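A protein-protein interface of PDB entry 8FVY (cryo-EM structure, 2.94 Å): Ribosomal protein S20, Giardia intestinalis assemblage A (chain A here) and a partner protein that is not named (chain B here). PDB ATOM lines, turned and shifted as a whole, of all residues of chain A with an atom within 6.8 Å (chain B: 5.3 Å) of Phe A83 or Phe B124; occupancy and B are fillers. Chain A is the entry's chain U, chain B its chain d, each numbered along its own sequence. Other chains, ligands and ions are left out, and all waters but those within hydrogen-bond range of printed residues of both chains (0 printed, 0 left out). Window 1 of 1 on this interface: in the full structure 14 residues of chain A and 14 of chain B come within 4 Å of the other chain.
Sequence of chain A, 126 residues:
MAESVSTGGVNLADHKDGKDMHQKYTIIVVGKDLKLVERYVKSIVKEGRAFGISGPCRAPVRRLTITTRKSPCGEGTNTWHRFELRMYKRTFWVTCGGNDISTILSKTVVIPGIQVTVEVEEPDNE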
ATOM      1  N   LEU A  64     -31.652  17.631 -16.759  1.00  0.00           N
ATOM      2  CA  LEU A  64     -31.248  18.792 -17.522  1.00  0.00           C
ATOM      3  C   LEU A  64     -30.272  18.362 -18.599  1.00  0.00           C
ATOM      4  O   LEU A  64     -29.333  17.615 -18.325  1.00  0.00           O
ATOM      5  CB  LEU A  64     -30.598  19.815 -16.607  1.00  0.00           C
ATOM      6  CG  LEU A  64     -31.509  20.711 -15.792  1.00  0.00           C
ATOM      7  CD1 LEU A  64     -32.570  19.922 -15.212  1.00  0.00           C
ATOM      8  CD2 LEU A  64     -30.722  21.339 -14.722  1.00  0.00           C
ATOM      9  N   THR A  65     -30.490  18.830 -19.817  1.00  0.00           N
ATOM     10  CA  THR A  65     -29.681  18.431 -20.951  1.00  0.00           C
ATOM     11  C   THR A  65     -29.064  19.641 -21.619  1.00  0.00           C
ATOM     12  O   THR A  65     -29.729  20.654 -21.844  1.00  0.00           O
ATOM     13  CB  THR A  65     -30.492  17.645 -21.968  1.00  0.00           C
ATOM     14  OG1 THR A  65     -31.565  18.456 -22.453  1.00  0.00           O
ATOM     15  CG2 THR A  65     -31.013  16.371 -21.355  1.00  0.00           C
ATOM     16  N   ILE A  66     -27.784  19.517 -21.928  1.00  0.00           N
ATOM     17  CA  ILE A  66     -27.041  20.539 -22.634  1.00  0.00           C
ATOM     18  C   ILE A  66     -26.153  19.856 -23.656  1.00  0.00           C
ATOM     19  O   ILE A  66     -25.346  18.990 -23.308  1.00  0.00           O
ATOM     20  CB  ILE A  66     -26.212  21.386 -21.662  1.00  0.00           C
ATOM     21  CG1 ILE A  66     -27.105  22.246 -20.793  1.00  0.00           C
ATOM     22  CG2 ILE A  66     -25.313  22.247 -22.397  1.00  0.00           C
ATOM     23  CD1 ILE A  66     -27.652  23.430 -21.472  1.00  0.00           C
ATOM     24  N   THR A  67     -26.287  20.238 -24.918  1.00  0.00           N
ATOM     25  CA  THR A  67     -25.415  19.752 -25.974  1.00  0.00           C
ATOM     26  C   THR A  67     -24.547  20.891 -26.468  1.00  0.00           C
ATOM     27  O   THR A  67     -25.045  21.979 -26.766  1.00  0.00           O
ATOM     28  CB  THR A  67     -26.204  19.153 -27.132  1.00  0.00           C
ATOM     29  OG1 THR A  67     -27.266  20.036 -27.507  1.00  0.00           O
ATOM     30  CG2 THR A  67     -26.743  17.828 -26.738  1.00  0.00           C
ATOM     31  N   THR A  68     -23.259  20.623 -26.563  1.00  0.00           N
ATOM     32  CA  THR A  68     -22.269  21.631 -26.851  1.00  0.00           C
ATOM     33  C   THR A  68     -21.290  21.084 -27.872  1.00  0.00           C
ATOM     34  O   THR A  68     -21.052  19.878 -27.949  1.00  0.00           O
ATOM     35  CB  THR A  68     -21.536  22.051 -25.576  1.00  0.00           C
ATOM     36  OG1 THR A  68     -22.459  22.626 -24.654  1.00  0.00           O
ATOM     37  CG2 THR A  68     -20.498  23.056 -25.870  1.00  0.00           C
ATOM     38  N   HIS A  81     -20.561  17.161 -27.270  1.00  0.00           N
ATOM     39  CA  HIS A  81     -20.637  16.756 -25.880  1.00  0.00           C
ATOM     40  C   HIS A  81     -22.092  16.553 -25.501  1.00  0.00           C
ATOM     41  O   HIS A  81     -22.985  17.179 -26.077  1.00  0.00           O
ATOM     42  CB  HIS A  81     -20.050  17.822 -24.970  1.00  0.00           C
ATOM     43  CG  HIS A  81     -18.583  17.701 -24.732  1.00  0.00           C
ATOM     44  ND1 HIS A  81     -17.955  16.497 -24.511  1.00  0.00           N
ATOM     45  CD2 HIS A  81     -17.622  18.648 -24.654  1.00  0.00           C
ATOM     46  CE1 HIS A  81     -16.665  16.709 -24.324  1.00  0.00           C
ATOM     47  NE2 HIS A  81     -16.438  18.005 -24.400  1.00  0.00           N
ATOM     48  N   ARG A  82     -22.328  15.704 -24.513  1.00  0.00           N
ATOM     49  CA  ARG A  82     -23.676  15.457 -24.017  1.00  0.00           C
ATOM     50  C   ARG A  82     -23.617  15.409 -22.497  1.00  0.00           C
ATOM     51  O   ARG A  82     -23.402  14.346 -21.910  1.00  0.00           O
ATOM     52  CB  ARG A  82     -24.244  14.179 -24.588  1.00  0.00           C
ATOM     53  CG  ARG A  82     -24.233  14.163 -26.075  1.00  0.00           C
ATOM     54  CD  ARG A  82     -25.258  13.219 -26.656  1.00  0.00           C
ATOM     55  NE  ARG A  82     -24.772  11.849 -26.710  1.00  0.00           N
ATOM     56  CZ  ARG A  82     -24.254  11.280 -27.790  1.00  0.00           C
ATOM     57  NH1 ARG A  82     -24.058  11.959 -28.905  1.00  0.00           N
ATOM     58  NH2 ARG A  82     -23.914   9.999 -27.748  1.00  0.00           N
ATOM     59  N   PHE A  83     -23.798  16.559 -21.870  1.00  0.00           N
ATOM     60  CA  PHE A  83     -23.890  16.659 -20.431  1.00  0.00           C
ATOM     61  C   PHE A  83     -25.322  16.445 -19.975  1.00  0.00           C
ATOM     62  O   PHE A  83     -26.269  16.514 -20.756  1.00  0.00           O
ATOM     63  CB  PHE A  83     -23.426  18.019 -19.967  1.00  0.00           C
ATOM     64  CG  PHE A  83     -22.079  18.395 -20.426  1.00  0.00           C
ATOM     65  CD1 PHE A  83     -20.968  17.812 -19.886  1.00  0.00           C
ATOM     66  CD2 PHE A  83     -21.923  19.357 -21.382  1.00  0.00           C
ATOM     67  CE1 PHE A  83     -19.729  18.171 -20.305  1.00  0.00           C
ATOM     68  CE2 PHE A  83     -20.683  19.722 -21.802  1.00  0.00           C
ATOM     69  CZ  PHE A  83     -19.584  19.125 -21.261  1.00  0.00           C
ATOM     70  N   GLU A  84     -25.478  16.184 -18.684  1.00  0.00           N
ATOM     71  CA  GLU A  84     -26.795  16.293 -18.087  1.00  0.00           C
ATOM     72  C   GLU A  84     -26.660  16.368 -16.576  1.00  0.00           C
ATOM     73  O   GLU A  84     -25.620  16.033 -16.008  1.00  0.00           O
ATOM     74  CB  GLU A  84     -27.705  15.136 -18.478  1.00  0.00           C
ATOM     75  CG  GLU A  84     -27.076  13.793 -18.442  1.00  0.00           C
ATOM     76  CD  GLU A  84     -28.071  12.733 -18.084  1.00  0.00           C
ATOM     77  OE1 GLU A  84     -29.279  13.016 -18.181  1.00  0.00           O
ATOM     78  OE2 GLU A  84     -27.657  11.622 -17.710  1.00  0.00           O
ATOM     79  N   LEU A  85     -27.738  16.816 -15.940  1.00  0.00           N
ATOM     80  CA  LEU A  85     -27.824  16.953 -14.491  1.00  0.00           C
ATOM     81  C   LEU A  85     -29.134  16.335 -14.032  1.00  0.00           C
ATOM     82  O   LEU A  85     -30.194  16.952 -14.136  1.00  0.00           O
ATOM     83  CB  LEU A  85     -27.747  18.384 -14.078  1.00  0.00           C
ATOM     84  CG  LEU A  85     -26.996  18.632 -12.790  1.00  0.00           C
ATOM     85  CD1 LEU A  85     -26.732  20.048 -12.631  1.00  0.00           C
ATOM     86  CD2 LEU A  85     -27.805  18.171 -11.674  1.00  0.00           C
ATOM     87  N   TYR B 112     -26.046  30.480 -23.100  1.00  0.00           N
ATOM     88  CA  TYR B 112     -27.123  29.588 -22.696  1.00  0.00           C
ATOM     89  C   TYR B 112     -27.982  30.262 -21.641  1.00  0.00           C
ATOM     90  O   TYR B 112     -27.624  30.312 -20.464  1.00  0.00           O
ATOM     91  CB  TYR B 112     -26.551  28.279 -22.180  1.00  0.00           C
ATOM     92  CG  TYR B 112     -26.124  27.331 -23.252  1.00  0.00           C
ATOM     93  CD1 TYR B 112     -27.033  26.820 -24.152  1.00  0.00           C
ATOM     94  CD2 TYR B 112     -24.813  26.946 -23.367  1.00  0.00           C
ATOM     95  CE1 TYR B 112     -26.641  25.955 -25.131  1.00  0.00           C
ATOM     96  CE2 TYR B 112     -24.413  26.089 -24.341  1.00  0.00           C
ATOM     97  CZ  TYR B 112     -25.326  25.595 -25.220  1.00  0.00           C
ATOM     98  OH  TYR B 112     -24.901  24.733 -26.191  1.00  0.00           O
ATOM     99  N   LEU B 117     -29.116  30.054 -16.641  1.00  0.00           N
ATOM    100  CA  LEU B 117     -27.682  29.883 -16.489  1.00  0.00           C
ATOM    101  C   LEU B 117     -26.920  31.159 -16.814  1.00  0.00           C
ATOM    102  O   LEU B 117     -26.384  31.819 -15.922  1.00  0.00           O
ATOM    103  CB  LEU B 117     -27.221  28.767 -17.407  1.00  0.00           C
ATOM    104  CG  LEU B 117     -27.281  27.341 -16.905  1.00  0.00           C
ATOM    105  CD1 LEU B 117     -26.857  26.454 -18.006  1.00  0.00           C
ATOM    106  CD2 LEU B 117     -26.395  27.133 -15.736  1.00  0.00           C
ATOM    107  N   ILE B 119     -24.244  31.391 -19.222  1.00  0.00           N
ATOM    108  CA  ILE B 119     -22.870  30.949 -19.352  1.00  0.00           C
ATOM    109  C   ILE B 119     -22.605  30.673 -20.819  1.00  0.00           C
ATOM    110  O   ILE B 119     -23.419  30.032 -21.489  1.00  0.00           O
ATOM    111  CB  ILE B 119     -22.610  29.695 -18.510  1.00  0.00           C
ATOM    112  CG1 ILE B 119     -23.029  29.935 -17.081  1.00  0.00           C
ATOM    113  CG2 ILE B 119     -21.187  29.385 -18.484  1.00  0.00           C
ATOM    114  CD1 ILE B 119     -23.022  28.731 -16.281  1.00  0.00           C
ATOM    115  N   CYS B 120     -21.484  31.170 -21.320  1.00  0.00           N
ATOM    116  CA  CYS B 120     -21.074  30.867 -22.678  1.00  0.00           C
ATOM    117  C   CYS B 120     -20.717  29.398 -22.830  1.00  0.00           C
ATOM    118  O   CYS B 120     -20.298  28.732 -21.884  1.00  0.00           O
ATOM    119  CB  CYS B 120     -19.887  31.727 -23.073  1.00  0.00           C
ATOM    120  SG  CYS B 120     -19.202  31.360 -24.675  1.00  0.00           S
ATOM    121  N   ARG B 121     -20.879  28.895 -24.048  1.00  0.00           N
ATOM    122  CA  ARG B 121     -20.613  27.490 -24.306  1.00  0.00           C
ATOM    123  C   ARG B 121     -19.151  27.149 -24.073  1.00  0.00           C
ATOM    124  O   ARG B 121     -18.820  26.037 -23.642  1.00  0.00           O
ATOM    125  CB  ARG B 121     -21.023  27.143 -25.731  1.00  0.00           C
ATOM    126  CG  ARG B 121     -20.085  27.639 -26.795  1.00  0.00           C
ATOM    127  CD  ARG B 121     -20.503  27.161 -28.154  1.00  0.00           C
ATOM    128  NE  ARG B 121     -19.587  27.564 -29.208  1.00  0.00           N
ATOM    129  CZ  ARG B 121     -18.489  26.906 -29.547  1.00  0.00           C
ATOM    130  NH1 ARG B 121     -18.103  25.825 -28.901  1.00  0.00           N
ATOM    131  NH2 ARG B 121     -17.763  27.341 -30.567  1.00  0.00           N
ATOM    132  N   ARG B 122     -18.258  28.072 -24.408  1.00  0.00           N
ATOM    133  CA  ARG B 122     -16.846  27.833 -24.172  1.00  0.00           C
ATOM    134  C   ARG B 122     -16.527  27.922 -22.693  1.00  0.00           C
ATOM    135  O   ARG B 122     -15.856  27.049 -22.142  1.00  0.00           O
ATOM    136  CB  ARG B 122     -16.028  28.842 -24.969  1.00  0.00           C
ATOM    137  CG  ARG B 122     -16.533  29.019 -26.365  1.00  0.00           C
ATOM    138  CD  ARG B 122     -15.484  29.592 -27.244  1.00  0.00           C
ATOM    139  NE  ARG B 122     -15.939  30.019 -28.560  1.00  0.00           N
ATOM    140  CZ  ARG B 122     -16.864  30.940 -28.790  1.00  0.00           C
ATOM    141  NH1 ARG B 122     -17.537  31.516 -27.809  1.00  0.00           N
ATOM    142  NH2 ARG B 122     -17.116  31.302 -30.039  1.00  0.00           N
ATOM    143  N   CYS B 123     -17.020  28.960 -22.034  1.00  0.00           N
ATOM    144  CA  CYS B 123     -16.825  29.187 -20.613  1.00  0.00           C
ATOM    145  C   CYS B 123     -17.588  28.182 -19.752  1.00  0.00           C
ATOM    146  O   CYS B 123     -17.677  28.378 -18.542  1.00  0.00           O
ATOM    147  CB  CYS B 123     -17.205  30.656 -20.302  1.00  0.00           C
ATOM    148  SG  CYS B 123     -15.875  31.868 -20.590  1.00  0.00           S
ATOM    149  N   PHE B 124     -18.069  27.081 -20.341  1.00  0.00           N
ATOM    150  CA  PHE B 124     -18.973  26.132 -19.708  1.00  0.00           C
ATOM    151  C   PHE B 124     -18.364  24.761 -19.480  1.00  0.00           C
ATOM    152  O   PHE B 124     -18.507  24.190 -18.396  1.00  0.00           O
ATOM    153  CB  PHE B 124     -20.217  25.984 -20.580  1.00  0.00           C
ATOM    154  CG  PHE B 124     -21.194  24.958 -20.095  1.00  0.00           C
ATOM    155  CD1 PHE B 124     -22.025  25.210 -19.038  1.00  0.00           C
ATOM    156  CD2 PHE B 124     -21.284  23.745 -20.716  1.00  0.00           C
ATOM    157  CE1 PHE B 124     -22.905  24.276 -18.607  1.00  0.00           C
ATOM    158  CE2 PHE B 124     -22.175  22.802 -20.276  1.00  0.00           C
ATOM    159  CZ  PHE B 124     -22.978  23.078 -19.223  1.00  0.00           C
ATOM    160  N   LYS B 125     -17.715  24.208 -20.500  1.00  0.00           N
ATOM    161  CA  LYS B 125     -17.083  22.901 -20.372  1.00  0.00           C
ATOM    162  C   LYS B 125     -16.109  22.851 -19.209  1.00  0.00           C
ATOM    163  O   LYS B 125     -15.917  21.790 -18.606  1.00  0.00           O
ATOM    164  CB  LYS B 125     -16.344  22.562 -21.647  1.00  0.00           C
ATOM    165  CG  LYS B 125     -17.211  22.499 -22.841  1.00  0.00           C
ATOM    166  CD  LYS B 125     -16.456  21.995 -24.058  1.00  0.00           C
ATOM    167  CE  LYS B 125     -15.526  23.043 -24.645  1.00  0.00           C
ATOM    168  NZ  LYS B 125     -16.221  23.928 -25.613  1.00  0.00           N
ATOM    169  N   GLU B 126     -15.459  23.969 -18.901  1.00  0.00           N
ATOM    170  CA  GLU B 126     -14.495  23.970 -17.815  1.00  0.00           C
ATOM    171  C   GLU B 126     -15.174  23.778 -16.467  1.00  0.00           C
ATOM    172  O   GLU B 126     -14.784  22.904 -15.686  1.00  0.00           O
ATOM    173  CB  GLU B 126     -13.703  25.274 -17.818  1.00  0.00           C
ATOM    174  CG  GLU B 126     -12.867  25.524 -19.055  1.00  0.00           C
ATOM    175  CD  GLU B 126     -13.695  25.870 -20.264  1.00  0.00           C
ATOM    176  OE1 GLU B 126     -14.850  26.300 -20.077  1.00  0.00           O
ATOM    177  OE2 GLU B 126     -13.192  25.725 -21.398  1.00  0.00           O
ATOM    178  N   ASN B 127     -16.203  24.566 -16.190  1.00  0.00           N
ATOM    179  CA  ASN B 127     -16.835  24.602 -14.884  1.00  0.00           C
ATOM    180  C   ASN B 127     -17.983  23.615 -14.748  1.00  0.00           C
ATOM    181  O   ASN B 127     -18.578  23.513 -13.668  1.00  0.00           O
ATOM    182  CB  ASN B 127     -17.324  26.021 -14.609  1.00  0.00           C
ATOM    183  CG  ASN B 127     -16.194  26.996 -14.416  1.00  0.00           C
ATOM    184  OD1 ASN B 127     -15.693  27.180 -13.311  1.00  0.00           O
ATOM    185  ND2 ASN B 127     -15.790  27.634 -15.493  1.00  0.00           N
ATOM    186  N   ALA B 128     -18.282  22.871 -15.805  1.00  0.00           N
ATOM    187  CA  ALA B 128     -19.421  21.972 -15.793  1.00  0.00           C
ATOM    188  C   ALA B 128     -19.284  20.883 -14.746  1.00  0.00           C
ATOM    189  O   ALA B 128     -20.271  20.511 -14.107  1.00  0.00           O
ATOM    190  CB  ALA B 128     -19.586  21.352 -17.160  1.00  0.00           C
ATOM    191  N   PHE B 133     -22.872  18.932 -13.807  1.00  0.00           N
ATOM    192  CA  PHE B 133     -23.069  18.315 -15.101  1.00  0.00           C
ATOM    193  C   PHE B 133     -21.976  17.296 -15.368  1.00  0.00           C
ATOM    194  O   PHE B 133     -20.791  17.566 -15.167  1.00  0.00           O
ATOM    195  CB  PHE B 133     -23.051  19.366 -16.184  1.00  0.00           C
ATOM    196  CG  PHE B 133     -24.255  20.222 -16.227  1.00  0.00           C
ATOM    197  CD1 PHE B 133     -24.372  21.310 -15.413  1.00  0.00           C
ATOM    198  CD2 PHE B 133     -25.265  19.948 -17.102  1.00  0.00           C
ATOM    199  CE1 PHE B 133     -25.473  22.098 -15.472  1.00  0.00           C
ATOM    200  CE2 PHE B 133     -26.363  20.732 -17.158  1.00  0.00           C
ATOM    201  CZ  PHE B 133     -26.469  21.807 -16.345  1.00  0.00           C
ATOM    202  N   VAL B 134     -22.376  16.125 -15.834  1.00  0.00           N
ATOM    203  CA  VAL B 134     -21.442  15.053 -16.121  1.00  0.00           C
ATOM    204  C   VAL B 134     -21.797  14.421 -17.451  1.00  0.00           C
ATOM    205  O   VAL B 134     -22.923  14.539 -17.940  1.00  0.00           O
ATOM    206  CB  VAL B 134     -21.436  13.994 -15.013  1.00  0.00           C
ATOM    207  CG1 VAL B 134     -20.898  14.596 -13.742  1.00  0.00           C
ATOM    208  CG2 VAL B 134     -22.822  13.443 -14.812  1.00  0.00           C
ATOM    209  N   LYS B 135     -20.828  13.726 -18.018  1.00  0.00           N
ATOM    210  CA  LYS B 135     -20.914  13.178 -19.361  1.00  0.00           C
ATOM    211  C   LYS B 135     -21.071  11.671 -19.242  1.00  0.00           C
ATOM    212  O   LYS B 135     -20.109  10.954 -18.958  1.00  0.00           O
ATOM    213  CB  LYS B 135     -19.677  13.547 -20.164  1.00  0.00           C
ATOM    214  CG  LYS B 135     -19.652  12.961 -21.542  1.00  0.00           C
ATOM    215  CD  LYS B 135     -18.903  13.803 -22.556  1.00  0.00           C
ATOM    216  CE  LYS B 135     -17.755  14.569 -21.961  1.00  0.00           C
ATOM    217  NZ  LYS B 135     -16.914  13.764 -21.063  1.00  0.00           N
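N of Glu A84 lies within hydrogen-bond range of O of Val B134 (3.1 Å). OH of Tyr B112 is in hydrogen-bond range of O of Thr A67 (2.8 Å).
The backbone NH of Phe B124 lies within hydrogen-bond range of the side-chain carboxylate of Glu B126. N of Tyr B112 lies within hydrogen-bond range of O of Ile B119, at 3.1 Å. The backbone carbonyl oxygen (O) of Ile A66 is in hydrogen-bond range of the backbone NH (N) of Phe A83 (3.2 Å). The backbone carbonyl oxygen (O) of Ala B128 lies within hydrogen-bond range of the backbone NH (N) of Phe B133 (3.1 Å). The backbone carbonyl oxygen of Leu A64 is in hydrogen-bond range of the backbone NH of Leu A85, at 3.0 Å. The backbone carbonyl oxygen of Thr A68 lies within hydrogen-bond range of the backbone NH of His A81 (2.8 Å).
Among the printed residues, merely in contact across the chains: Ile A66 with Phe B124 (3.8 Å), Thr A68 with Tyr B112 (3.6 Å), His A81 with Lys B125 (3.6 Å), His A81 with Lys B135 (3.2 Å), Arg A82 with Lys B135 (3.7 Å), Phe A83 with Phe B124 (3.6 Å), Phe A83 with Phe B133 (3.9 Å), Phe A83 with Val B134 (3.4 Å), Glu A84 with Phe B133 (3.5 Å) and Leu A85 with Phe B133 (3.7 Å).
Phe A83 touches just these residues of chain B: Phe B124, Phe B133 and Val B134. Of chain A, only Ile A66 and Phe A83 come within 4 Å of Phe B124. Printed residues of chain B within 4 Å of His A81: Lys B125 (3.6 Å) and Lys B135 (3.2 Å). Of the printed residues of chain B, Arg A82 touches Lys B135 (3.7 Å). Of the printed residues of chain B, Ile A66 touches Phe B124 (3.8 Å). Ala B128 touches none of the printed residues of chain A. The nearest printed residue of chain B that does not touch Phe A83 is Lys B125 (4.4 Å). The nearest residue of chain A that does not touch Phe B124 is Thr A68 (4.3 Å).
Hydrophobic or aromatic side chains of chain B within 4 Å of the printed part of chain A: Tyr B112, Phe B124, Phe B133 and Val B134. Among the printed residues, 12 pairs touch across the chains. Among the printed residues, no Asp or Glu carboxylate lies within 4 Å of a Lys or Arg side-chain nitrogen of the other chain.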
